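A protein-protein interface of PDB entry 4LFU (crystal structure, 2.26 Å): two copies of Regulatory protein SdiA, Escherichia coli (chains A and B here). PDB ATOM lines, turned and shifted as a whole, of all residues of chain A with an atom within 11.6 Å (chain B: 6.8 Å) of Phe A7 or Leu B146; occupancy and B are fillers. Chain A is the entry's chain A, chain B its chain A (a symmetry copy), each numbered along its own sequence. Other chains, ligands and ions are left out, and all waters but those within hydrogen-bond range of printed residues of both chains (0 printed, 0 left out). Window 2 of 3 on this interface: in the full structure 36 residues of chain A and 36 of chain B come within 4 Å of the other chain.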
ATOM      1  N   ASP A   5     -30.883 -26.610 -22.411  1.00  0.00           N
ATOM      2  CA  ASP A   5     -29.821 -25.559 -22.352  1.00  0.00           C
ATOM      3  C   ASP A   5     -29.588 -24.962 -23.749  1.00  0.00           C
ATOM      4  O   ASP A   5     -29.189 -25.674 -24.684  1.00  0.00           O
ATOM      5  CB  ASP A   5     -28.537 -26.163 -21.770  1.00  0.00           C
ATOM      6  CG  ASP A   5     -27.405 -25.160 -21.653  1.00  0.00           C
ATOM      7  OD1 ASP A   5     -26.353 -25.401 -22.282  1.00  0.00           O
ATOM      8  OD2 ASP A   5     -27.561 -24.150 -20.936  1.00  0.00           O
ATOM      9  N   PHE A   6     -29.855 -23.658 -23.885  1.00  0.00           N
ATOM     10  CA  PHE A   6     -29.787 -22.987 -25.184  1.00  0.00           C
ATOM     11  C   PHE A   6     -28.364 -22.912 -25.742  1.00  0.00           C
ATOM     12  O   PHE A   6     -28.157 -23.154 -26.930  1.00  0.00           O
ATOM     13  CB  PHE A   6     -30.437 -21.585 -25.171  1.00  0.00           C
ATOM     14  CG  PHE A   6     -30.338 -20.875 -26.509  1.00  0.00           C
ATOM     15  CD1 PHE A   6     -31.192 -21.224 -27.569  1.00  0.00           C
ATOM     16  CD2 PHE A   6     -29.349 -19.906 -26.734  1.00  0.00           C
ATOM     17  CE1 PHE A   6     -31.078 -20.595 -28.821  1.00  0.00           C
ATOM     18  CE2 PHE A   6     -29.232 -19.274 -27.971  1.00  0.00           C
ATOM     19  CZ  PHE A   6     -30.104 -19.619 -29.020  1.00  0.00           C
ATOM     20  N   PHE A   7     -27.402 -22.570 -24.885  1.00  0.00           N
ATOM     21  CA  PHE A   7     -25.985 -22.511 -25.264  1.00  0.00           C
ATOM     22  C   PHE A   7     -25.485 -23.801 -25.921  1.00  0.00           C
ATOM     23  O   PHE A   7     -24.696 -23.748 -26.863  1.00  0.00           O
ATOM     24  CB  PHE A   7     -25.114 -22.173 -24.043  1.00  0.00           C
ATOM     25  CG  PHE A   7     -25.135 -20.714 -23.639  1.00  0.00           C
ATOM     26  CD1 PHE A   7     -26.110 -19.840 -24.117  1.00  0.00           C
ATOM     27  CD2 PHE A   7     -24.190 -20.226 -22.746  1.00  0.00           C
ATOM     28  CE1 PHE A   7     -26.128 -18.490 -23.733  1.00  0.00           C
ATOM     29  CE2 PHE A   7     -24.198 -18.878 -22.346  1.00  0.00           C
ATOM     30  CZ  PHE A   7     -25.176 -18.009 -22.842  1.00  0.00           C
ATOM     31  N   SER A   8     -25.936 -24.956 -25.428  1.00  0.00           N
ATOM     32  CA  SER A   8     -25.527 -26.239 -26.016  1.00  0.00           C
ATOM     33  C   SER A   8     -26.301 -26.546 -27.291  1.00  0.00           C
ATOM     34  O   SER A   8     -25.713 -26.981 -28.291  1.00  0.00           O
ATOM     35  CB  SER A   8     -25.623 -27.399 -25.012  1.00  0.00           C
ATOM     36  OG  SER A   8     -26.960 -27.645 -24.599  1.00  0.00           O
ATOM     37  N   TRP A   9     -27.613 -26.309 -27.258  1.00  0.00           N
ATOM     38  CA  TRP A   9     -28.441 -26.404 -28.460  1.00  0.00           C
ATOM     39  C   TRP A   9     -27.794 -25.630 -29.602  1.00  0.00           C
ATOM     40  O   TRP A   9     -27.560 -26.186 -30.680  1.00  0.00           O
ATOM     41  CB  TRP A   9     -29.877 -25.900 -28.198  1.00  0.00           C
ATOM     42  CG  TRP A   9     -30.777 -26.087 -29.417  1.00  0.00           C
ATOM     43  CD1 TRP A   9     -31.487 -27.209 -29.748  1.00  0.00           C
ATOM     44  CD2 TRP A   9     -31.021 -25.133 -30.464  1.00  0.00           C
ATOM     45  NE1 TRP A   9     -32.162 -27.011 -30.926  1.00  0.00           N
ATOM     46  CE2 TRP A   9     -31.898 -25.746 -31.388  1.00  0.00           C
ATOM     47  CE3 TRP A   9     -30.597 -23.822 -30.702  1.00  0.00           C
ATOM     48  CZ2 TRP A   9     -32.353 -25.087 -32.550  1.00  0.00           C
ATOM     49  CZ3 TRP A   9     -31.054 -23.163 -31.861  1.00  0.00           C
ATOM     50  CH2 TRP A   9     -31.914 -23.803 -32.771  1.00  0.00           C
ATOM     51  N   ARG A  10     -27.476 -24.362 -29.346  1.00  0.00           N
ATOM     52  CA  ARG A  10     -26.866 -23.477 -30.347  1.00  0.00           C
ATOM     53  C   ARG A  10     -25.537 -24.012 -30.879  1.00  0.00           C
ATOM     54  O   ARG A  10     -25.273 -23.938 -32.077  1.00  0.00           O
ATOM     55  CB  ARG A  10     -26.699 -22.053 -29.784  1.00  0.00           C
ATOM     56  CG  ARG A  10     -26.146 -21.019 -30.780  1.00  0.00           C
ATOM     57  CD  ARG A  10     -25.992 -19.625 -30.159  1.00  0.00           C
ATOM     58  NE  ARG A  10     -24.582 -19.276 -29.964  1.00  0.00           N
ATOM     59  CZ  ARG A  10     -23.850 -18.577 -30.831  1.00  0.00           C
ATOM     60  NH1 ARG A  10     -24.382 -18.131 -31.963  1.00  0.00           N
ATOM     61  NH2 ARG A  10     -22.581 -18.321 -30.565  1.00  0.00           N
ATOM     62  N   ARG A  11     -24.712 -24.544 -29.976  1.00  0.00           N
ATOM     63  CA  ARG A  11     -23.396 -25.099 -30.309  1.00  0.00           C
ATOM     64  C   ARG A  11     -23.515 -26.281 -31.301  1.00  0.00           C
ATOM     65  O   ARG A  11     -22.815 -26.328 -32.323  1.00  0.00           O
ATOM     66  CB  ARG A  11     -22.664 -25.505 -29.009  1.00  0.00           C
ATOM     67  CG  ARG A  11     -21.168 -25.210 -28.967  1.00  0.00           C
ATOM     68  CD  ARG A  11     -20.640 -24.901 -27.519  1.00  0.00           C
ATOM     69  NE  ARG A  11     -21.230 -25.739 -26.463  1.00  0.00           N
ATOM     70  CZ  ARG A  11     -21.865 -25.279 -25.381  1.00  0.00           C
ATOM     71  NH1 ARG A  11     -21.986 -23.968 -25.167  1.00  0.00           N
ATOM     72  NH2 ARG A  11     -22.381 -26.134 -24.497  1.00  0.00           N
ATOM     73  N   THR A  12     -24.429 -27.206 -31.004  1.00  0.00           N
ATOM     74  CA  THR A  12     -24.742 -28.338 -31.892  1.00  0.00           C
ATOM     75  C   THR A  12     -25.272 -27.917 -33.274  1.00  0.00           C
ATOM     76  O   THR A  12     -24.889 -28.493 -34.297  1.00  0.00           O
ATOM     77  CB  THR A  12     -25.795 -29.271 -31.247  1.00  0.00           C
ATOM     78  OG1 THR A  12     -25.507 -29.436 -29.854  1.00  0.00           O
ATOM     79  CG2 THR A  12     -25.826 -30.627 -31.949  1.00  0.00           C
ATOM     80  N   MET A  13     -26.154 -26.920 -33.299  1.00  0.00           N
ATOM     81  CA  MET A  13     -26.813 -26.533 -34.550  1.00  0.00           C
ATOM     82  C   MET A  13     -25.867 -25.860 -35.534  1.00  0.00           C
ATOM     83  O   MET A  13     -25.903 -26.163 -36.729  1.00  0.00           O
ATOM     84  CB  MET A  13     -28.074 -25.689 -34.291  1.00  0.00           C
ATOM     85  CG  MET A  13     -29.194 -26.443 -33.580  1.00  0.00           C
ATOM     86  SD  MET A  13     -29.639 -28.047 -34.332  1.00  0.00           S
ATOM     87  CE  MET A  13     -30.271 -27.515 -35.926  1.00  0.00           C
ATOM     88  N   LEU A  14     -25.021 -24.956 -35.035  1.00  0.00           N
ATOM     89  CA  LEU A  14     -23.984 -24.324 -35.857  1.00  0.00           C
ATOM     90  C   LEU A  14     -23.111 -25.377 -36.504  1.00  0.00           C
ATOM     91  O   LEU A  14     -22.820 -25.310 -37.699  1.00  0.00           O
ATOM     92  CB  LEU A  14     -23.120 -23.375 -35.021  1.00  0.00           C
ATOM     93  CG  LEU A  14     -23.883 -22.162 -34.499  1.00  0.00           C
ATOM     94  CD1 LEU A  14     -23.052 -21.355 -33.519  1.00  0.00           C
ATOM     95  CD2 LEU A  14     -24.350 -21.299 -35.668  1.00  0.00           C
ATOM     96  N   LEU A  15     -22.708 -26.367 -35.718  1.00  0.00           N
ATOM     97  CA  LEU A  15     -21.856 -27.423 -36.241  1.00  0.00           C
ATOM     98  C   LEU A  15     -22.583 -28.273 -37.280  1.00  0.00           C
ATOM     99  O   LEU A  15     -22.021 -28.553 -38.340  1.00  0.00           O
ATOM    100  CB  LEU A  15     -21.261 -28.271 -35.106  1.00  0.00           C
ATOM    101  CG  LEU A  15     -19.931 -27.739 -34.549  1.00  0.00           C
ATOM    102  CD1 LEU A  15     -19.638 -28.266 -33.118  1.00  0.00           C
ATOM    103  CD2 LEU A  15     -18.755 -28.060 -35.523  1.00  0.00           C
ATOM    104  N   ARG A  16     -23.827 -28.660 -36.990  1.00  0.00           N
ATOM    105  CA  ARG A  16     -24.640 -29.413 -37.947  1.00  0.00           C
ATOM    106  C   ARG A  16     -24.816 -28.714 -39.282  1.00  0.00           C
ATOM    107  O   ARG A  16     -24.683 -29.340 -40.308  1.00  0.00           O
ATOM    108  CB  ARG A  16     -26.008 -29.763 -37.367  1.00  0.00           C
ATOM    109  CG  ARG A  16     -26.125 -31.187 -36.882  1.00  0.00           C
ATOM    110  CD  ARG A  16     -27.556 -31.505 -36.543  1.00  0.00           C
ATOM    111  NE  ARG A  16     -27.636 -32.143 -35.235  1.00  0.00           N
ATOM    112  CZ  ARG A  16     -28.731 -32.194 -34.485  1.00  0.00           C
ATOM    113  NH1 ARG A  16     -29.865 -31.636 -34.906  1.00  0.00           N
ATOM    114  NH2 ARG A  16     -28.688 -32.800 -33.301  1.00  0.00           N
ATOM    115  N   ASP A 148     -39.175 -16.472 -25.796  1.00  0.00           N
ATOM    116  CA  ASP A 148     -37.766 -16.109 -25.950  1.00  0.00           C
ATOM    117  C   ASP A 148     -36.973 -17.274 -26.561  1.00  0.00           C
ATOM    118  O   ASP A 148     -36.143 -17.090 -27.455  1.00  0.00           O
ATOM    119  CB  ASP A 148     -37.167 -15.723 -24.575  1.00  0.00           C
ATOM    120  CG  ASP A 148     -38.109 -14.849 -23.709  1.00  0.00           C
ATOM    121  OD1 ASP A 148     -39.351 -15.094 -23.677  1.00  0.00           O
ATOM    122  OD2 ASP A 148     -37.593 -13.924 -23.023  1.00  0.00           O
ATOM    123  N   GLU A 149     -37.237 -18.477 -26.070  1.00  0.00           N
ATOM    124  CA  GLU A 149     -36.603 -19.673 -26.586  1.00  0.00           C
ATOM    125  C   GLU A 149     -36.924 -19.881 -28.070  1.00  0.00           C
ATOM    126  O   GLU A 149     -36.009 -20.026 -28.887  1.00  0.00           O
ATOM    127  CB  GLU A 149     -37.020 -20.886 -25.762  1.00  0.00           C
ATOM    128  CG  GLU A 149     -36.163 -22.118 -25.994  1.00  0.00           C
ATOM    129  CD  GLU A 149     -36.789 -23.390 -25.435  1.00  0.00           C
ATOM    130  OE1 GLU A 149     -36.848 -24.399 -26.177  1.00  0.00           O
ATOM    131  OE2 GLU A 149     -37.231 -23.390 -24.259  1.00  0.00           O
ATOM    132  N   LEU A 152     -35.205 -17.192 -30.351  1.00  0.00           N
ATOM    133  CA  LEU A 152     -33.766 -17.354 -30.473  1.00  0.00           C
ATOM    134  C   LEU A 152     -33.401 -18.586 -31.309  1.00  0.00           C
ATOM    135  O   LEU A 152     -32.421 -18.553 -32.081  1.00  0.00           O
ATOM    136  CB  LEU A 152     -33.109 -17.415 -29.088  1.00  0.00           C
ATOM    137  CG  LEU A 152     -32.928 -16.094 -28.319  1.00  0.00           C
ATOM    138  CD1 LEU A 152     -32.596 -16.394 -26.864  1.00  0.00           C
ATOM    139  CD2 LEU A 152     -31.841 -15.236 -28.927  1.00  0.00           C
ATOM    140  N   LYS A 153     -34.209 -19.645 -31.182  1.00  0.00           N
ATOM    141  CA  LYS A 153     -34.011 -20.868 -31.955  1.00  0.00           C
ATOM    142  C   LYS A 153     -34.287 -20.665 -33.423  1.00  0.00           C
ATOM    143  O   LYS A 153     -33.530 -21.128 -34.265  1.00  0.00           O
ATOM    144  CB  LYS A 153     -34.850 -22.019 -31.404  1.00  0.00           C
ATOM    145  CG  LYS A 153     -34.251 -22.620 -30.148  1.00  0.00           C
ATOM    146  CD  LYS A 153     -35.014 -23.837 -29.696  1.00  0.00           C
ATOM    147  CE  LYS A 153     -34.379 -24.431 -28.440  1.00  0.00           C
ATOM    148  NZ  LYS A 153     -34.975 -25.769 -28.171  1.00  0.00           N
ATOM    149  N   LEU A 156     -31.519 -18.571 -35.244  1.00  0.00           N
ATOM    150  CA  LEU A 156     -30.400 -19.409 -35.725  1.00  0.00           C
ATOM    151  C   LEU A 156     -30.756 -20.259 -36.942  1.00  0.00           C
ATOM    152  O   LEU A 156     -29.979 -20.315 -37.901  1.00  0.00           O
ATOM    153  CB  LEU A 156     -29.834 -20.285 -34.582  1.00  0.00           C
ATOM    154  CG  LEU A 156     -28.607 -21.197 -34.763  1.00  0.00           C
ATOM    155  CD1 LEU A 156     -28.063 -21.628 -33.393  1.00  0.00           C
ATOM    156  CD2 LEU A 156     -28.892 -22.460 -35.641  1.00  0.00           C
ATOM    157  N   PHE B   6     -29.386 -15.564 -19.364  1.00  0.00           N
ATOM    158  CA  PHE B   6     -29.367 -14.813 -20.620  1.00  0.00           C
ATOM    159  C   PHE B   6     -30.757 -14.338 -21.050  1.00  0.00           C
ATOM    160  O   PHE B   6     -30.911 -13.196 -21.480  1.00  0.00           O
ATOM    161  CB  PHE B   6     -28.679 -15.582 -21.770  1.00  0.00           C
ATOM    162  CG  PHE B   6     -28.690 -14.817 -23.082  1.00  0.00           C
ATOM    163  CD1 PHE B   6     -27.793 -13.757 -23.299  1.00  0.00           C
ATOM    164  CD2 PHE B   6     -29.637 -15.109 -24.073  1.00  0.00           C
ATOM    165  CE1 PHE B   6     -27.824 -13.023 -24.496  1.00  0.00           C
ATOM    166  CE2 PHE B   6     -29.673 -14.389 -25.266  1.00  0.00           C
ATOM    167  CZ  PHE B   6     -28.759 -13.341 -25.480  1.00  0.00           C
ATOM    168  N   ILE B 143      -9.668 -12.755 -18.588  1.00  0.00           N
ATOM    169  CA  ILE B 143     -10.965 -12.624 -17.927  1.00  0.00           C
ATOM    170  C   ILE B 143     -11.799 -13.873 -18.250  1.00  0.00           C
ATOM    171  O   ILE B 143     -11.835 -14.328 -19.410  1.00  0.00           O
ATOM    172  CB  ILE B 143     -11.720 -11.314 -18.322  1.00  0.00           C
ATOM    173  CG1 ILE B 143     -12.267 -11.392 -19.762  1.00  0.00           C
ATOM    174  CG2 ILE B 143     -10.812 -10.082 -18.105  1.00  0.00           C
ATOM    175  CD1 ILE B 143     -13.698 -10.861 -19.931  1.00  0.00           C
ATOM    176  N   PRO B 144     -12.452 -14.455 -17.226  1.00  0.00           N
ATOM    177  CA  PRO B 144     -13.260 -15.628 -17.545  1.00  0.00           C
ATOM    178  C   PRO B 144     -14.623 -15.200 -18.112  1.00  0.00           C
ATOM    179  O   PRO B 144     -15.447 -14.624 -17.393  1.00  0.00           O
ATOM    180  CB  PRO B 144     -13.400 -16.347 -16.185  1.00  0.00           C
ATOM    181  CG  PRO B 144     -12.699 -15.455 -15.148  1.00  0.00           C
ATOM    182  CD  PRO B 144     -12.512 -14.114 -15.792  1.00  0.00           C
ATOM    183  N   ILE B 145     -14.836 -15.434 -19.405  1.00  0.00           N
ATOM    184  CA  ILE B 145     -16.156 -15.210 -20.017  1.00  0.00           C
ATOM    185  C   ILE B 145     -16.477 -16.243 -21.098  1.00  0.00           C
ATOM    186  O   ILE B 145     -15.666 -16.506 -21.990  1.00  0.00           O
ATOM    187  CB  ILE B 145     -16.374 -13.740 -20.527  1.00  0.00           C
ATOM    188  CG1 ILE B 145     -17.872 -13.453 -20.701  1.00  0.00           C
ATOM    189  CG2 ILE B 145     -15.587 -13.470 -21.814  1.00  0.00           C
ATOM    190  CD1 ILE B 145     -18.266 -12.007 -20.530  1.00  0.00           C
ATOM    191  N   LEU B 146     -17.666 -16.828 -20.991  1.00  0.00           N
ATOM    192  CA  LEU B 146     -18.152 -17.809 -21.947  1.00  0.00           C
ATOM    193  C   LEU B 146     -18.230 -17.165 -23.340  1.00  0.00           C
ATOM    194  O   LEU B 146     -18.873 -16.132 -23.508  1.00  0.00           O
ATOM    195  CB  LEU B 146     -19.530 -18.297 -21.497  1.00  0.00           C
ATOM    196  CG  LEU B 146     -19.883 -19.785 -21.458  1.00  0.00           C
ATOM    197  CD1 LEU B 146     -21.122 -19.969 -20.585  1.00  0.00           C
ATOM    198  CD2 LEU B 146     -20.117 -20.357 -22.840  1.00  0.00           C
ATOM    199  N   SER B 147     -17.551 -17.765 -24.317  1.00  0.00           N
ATOM    200  CA  SER B 147     -17.492 -17.252 -25.689  1.00  0.00           C
ATOM    201  C   SER B 147     -18.895 -17.041 -26.278  1.00  0.00           C
ATOM    202  O   SER B 147     -19.163 -16.034 -26.941  1.00  0.00           O
ATOM    203  CB  SER B 147     -16.693 -18.220 -26.561  1.00  0.00           C
ATOM    204  OG  SER B 147     -16.524 -17.717 -27.876  1.00  0.00           O
ATOM    205  N   ASP B 148     -19.779 -17.997 -25.993  1.00  0.00           N
ATOM    206  CA  ASP B 148     -21.167 -18.017 -26.455  1.00  0.00           C
ATOM    207  C   ASP B 148     -21.961 -16.861 -25.827  1.00  0.00           C
ATOM    208  O   ASP B 148     -22.738 -16.175 -26.496  1.00  0.00           O
ATOM    209  CB  ASP B 148     -21.825 -19.371 -26.091  1.00  0.00           C
ATOM    210  CG  ASP B 148     -20.903 -20.595 -26.330  1.00  0.00           C
ATOM    211  OD1 ASP B 148     -19.673 -20.527 -26.041  1.00  0.00           O
ATOM    212  OD2 ASP B 148     -21.428 -21.650 -26.781  1.00  0.00           O
ATOM    213  N   GLU B 149     -21.756 -16.651 -24.534  1.00  0.00           N
ATOM    214  CA  GLU B 149     -22.397 -15.564 -23.823  1.00  0.00           C
ATOM    215  C   GLU B 149     -22.006 -14.204 -24.409  1.00  0.00           C
ATOM    216  O   GLU B 149     -22.882 -13.407 -24.762  1.00  0.00           O
ATOM    217  CB  GLU B 149     -22.057 -15.636 -22.338  1.00  0.00           C
ATOM    218  CG  GLU B 149     -22.936 -14.765 -21.457  1.00  0.00           C
ATOM    219  CD  GLU B 149     -22.376 -14.587 -20.051  1.00  0.00           C
ATOM    220  OE1 GLU B 149     -22.308 -13.427 -19.582  1.00  0.00           O
ATOM    221  OE2 GLU B 149     -21.995 -15.599 -19.411  1.00  0.00           O
ATOM    222  N   LEU B 150     -20.700 -13.943 -24.511  1.00  0.00           N
ATOM    223  CA  LEU B 150     -20.174 -12.693 -25.097  1.00  0.00           C
ATOM    224  C   LEU B 150     -20.686 -12.440 -26.525  1.00  0.00           C
ATOM    225  O   LEU B 150     -21.028 -11.321 -26.873  1.00  0.00           O
ATOM    226  CB  LEU B 150     -18.628 -12.662 -25.063  1.00  0.00           C
ATOM    227  CG  LEU B 150     -17.902 -11.472 -25.718  1.00  0.00           C
ATOM    228  CD1 LEU B 150     -18.166 -10.208 -24.937  1.00  0.00           C
ATOM    229  CD2 LEU B 150     -16.394 -11.708 -25.847  1.00  0.00           C
ATOM    230  N   GLN B 151     -20.742 -13.490 -27.333  1.00  0.00           N
ATOM    231  CA  GLN B 151     -21.232 -13.396 -28.702  1.00  0.00           C
ATOM    232  C   GLN B 151     -22.693 -12.976 -28.780  1.00  0.00           C
ATOM    233  O   GLN B 151     -23.034 -12.061 -29.535  1.00  0.00           O
ATOM    234  CB  GLN B 151     -21.043 -14.719 -29.417  1.00  0.00           C
ATOM    235  CG  GLN B 151     -19.617 -14.942 -29.822  1.00  0.00           C
ATOM    236  CD  GLN B 151     -19.468 -16.104 -30.749  1.00  0.00           C
ATOM    237  OE1 GLN B 151     -18.820 -17.100 -30.403  1.00  0.00           O
ATOM    238  NE2 GLN B 151     -20.073 -16.003 -31.941  1.00  0.00           N
ATOM    239  N   LEU B 152     -23.529 -13.635 -27.979  1.00  0.00           N
ATOM    240  CA  LEU B 152     -24.964 -13.405 -27.980  1.00  0.00           C
ATOM    241  C   LEU B 152     -25.321 -12.036 -27.392  1.00  0.00           C
ATOM    242  O   LEU B 152     -26.259 -11.369 -27.875  1.00  0.00           O
ATOM    243  CB  LEU B 152     -25.692 -14.531 -27.234  1.00  0.00           C
ATOM    244  CG  LEU B 152     -25.875 -15.875 -27.960  1.00  0.00           C
ATOM    245  CD1 LEU B 152     -26.289 -16.943 -26.958  1.00  0.00           C
ATOM    246  CD2 LEU B 152     -26.904 -15.780 -29.064  1.00  0.00           C
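NH1 of Arg A11 lies within salt-bridge range of OD2 of Asp B148.
The side-chain hydroxyl (OG) of Ser B147 lies within hydrogen-bond range of the side-chain amide oxygen (OE1) of Gln B151 (3.5 Å).
O of Phe A7 lies within hydrogen-bond range of NH1 of Arg A11, 3.2 Å away.
Phe A6 touches Leu B152 (CE2 to CD1, 3.9 Å).
Phe A7 touches Leu B146 (CE2 to CD1, 3.7 Å).
OD2 of Asp B148 touches O of Phe A7 (3.9 Å).
CA of Glu B149 touches CZ of Phe A7, at 3.8 Å.
CE1 of Phe A7 touches CD1 of Leu B152 (3.6 Å).
Gln B151 touches Arg A10.
Phe B6 touches Leu A152.
Of the printed residues of chain B, Phe A7 touches Leu B146, Asp B148, Glu B149 and Leu B152.
Leu B146 touches one residue of chain A.
Printed residues of chain A within 4 Å of Phe B6: Leu A152.
Of chain A, only Phe A7 and Arg A11 come within 4 Å of Asp B148.
Glu B149 touches just one residue of chain A: Phe A7.
No residue of chain A comes within 4 Å of Leu B150.
Of the printed residues of chain B, Phe A6 touches Leu B152.
Of the printed residues of chain B, Arg A11 touches Asp B148 (2.9 Å).
Leu A15 touches none of the printed residues of chain B.
Glu A149 touches none of the printed residues of chain B.
The nearest residue of chain B that does not touch Phe A7 is Phe B6 (4.3 Å).
Printed residues of chain A that touch a printed residue of chain B: Phe A6, Phe A7, Arg A10, Arg A11 and Leu A152.
Of the 11 printed residues of chain B, 6 touch a printed residue of chain A.
Hydrophobic or aromatic side chains of chain B that line the printed part of chain A: Phe B6, Leu B146 and Leu B152.
Among the printed residues, Asp or Glu carboxylates within 4 Å of a Lys or Arg side-chain nitrogen of the other chain: Arg A11 with Asp B148.
Phe A6 touches Leu B152, and with the chains exchanged Leu A152 touches Phe B6.
Of the 8 pairs that touch across the chains among the printed residues, 2 have their exchanged pair printed and touching as well.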
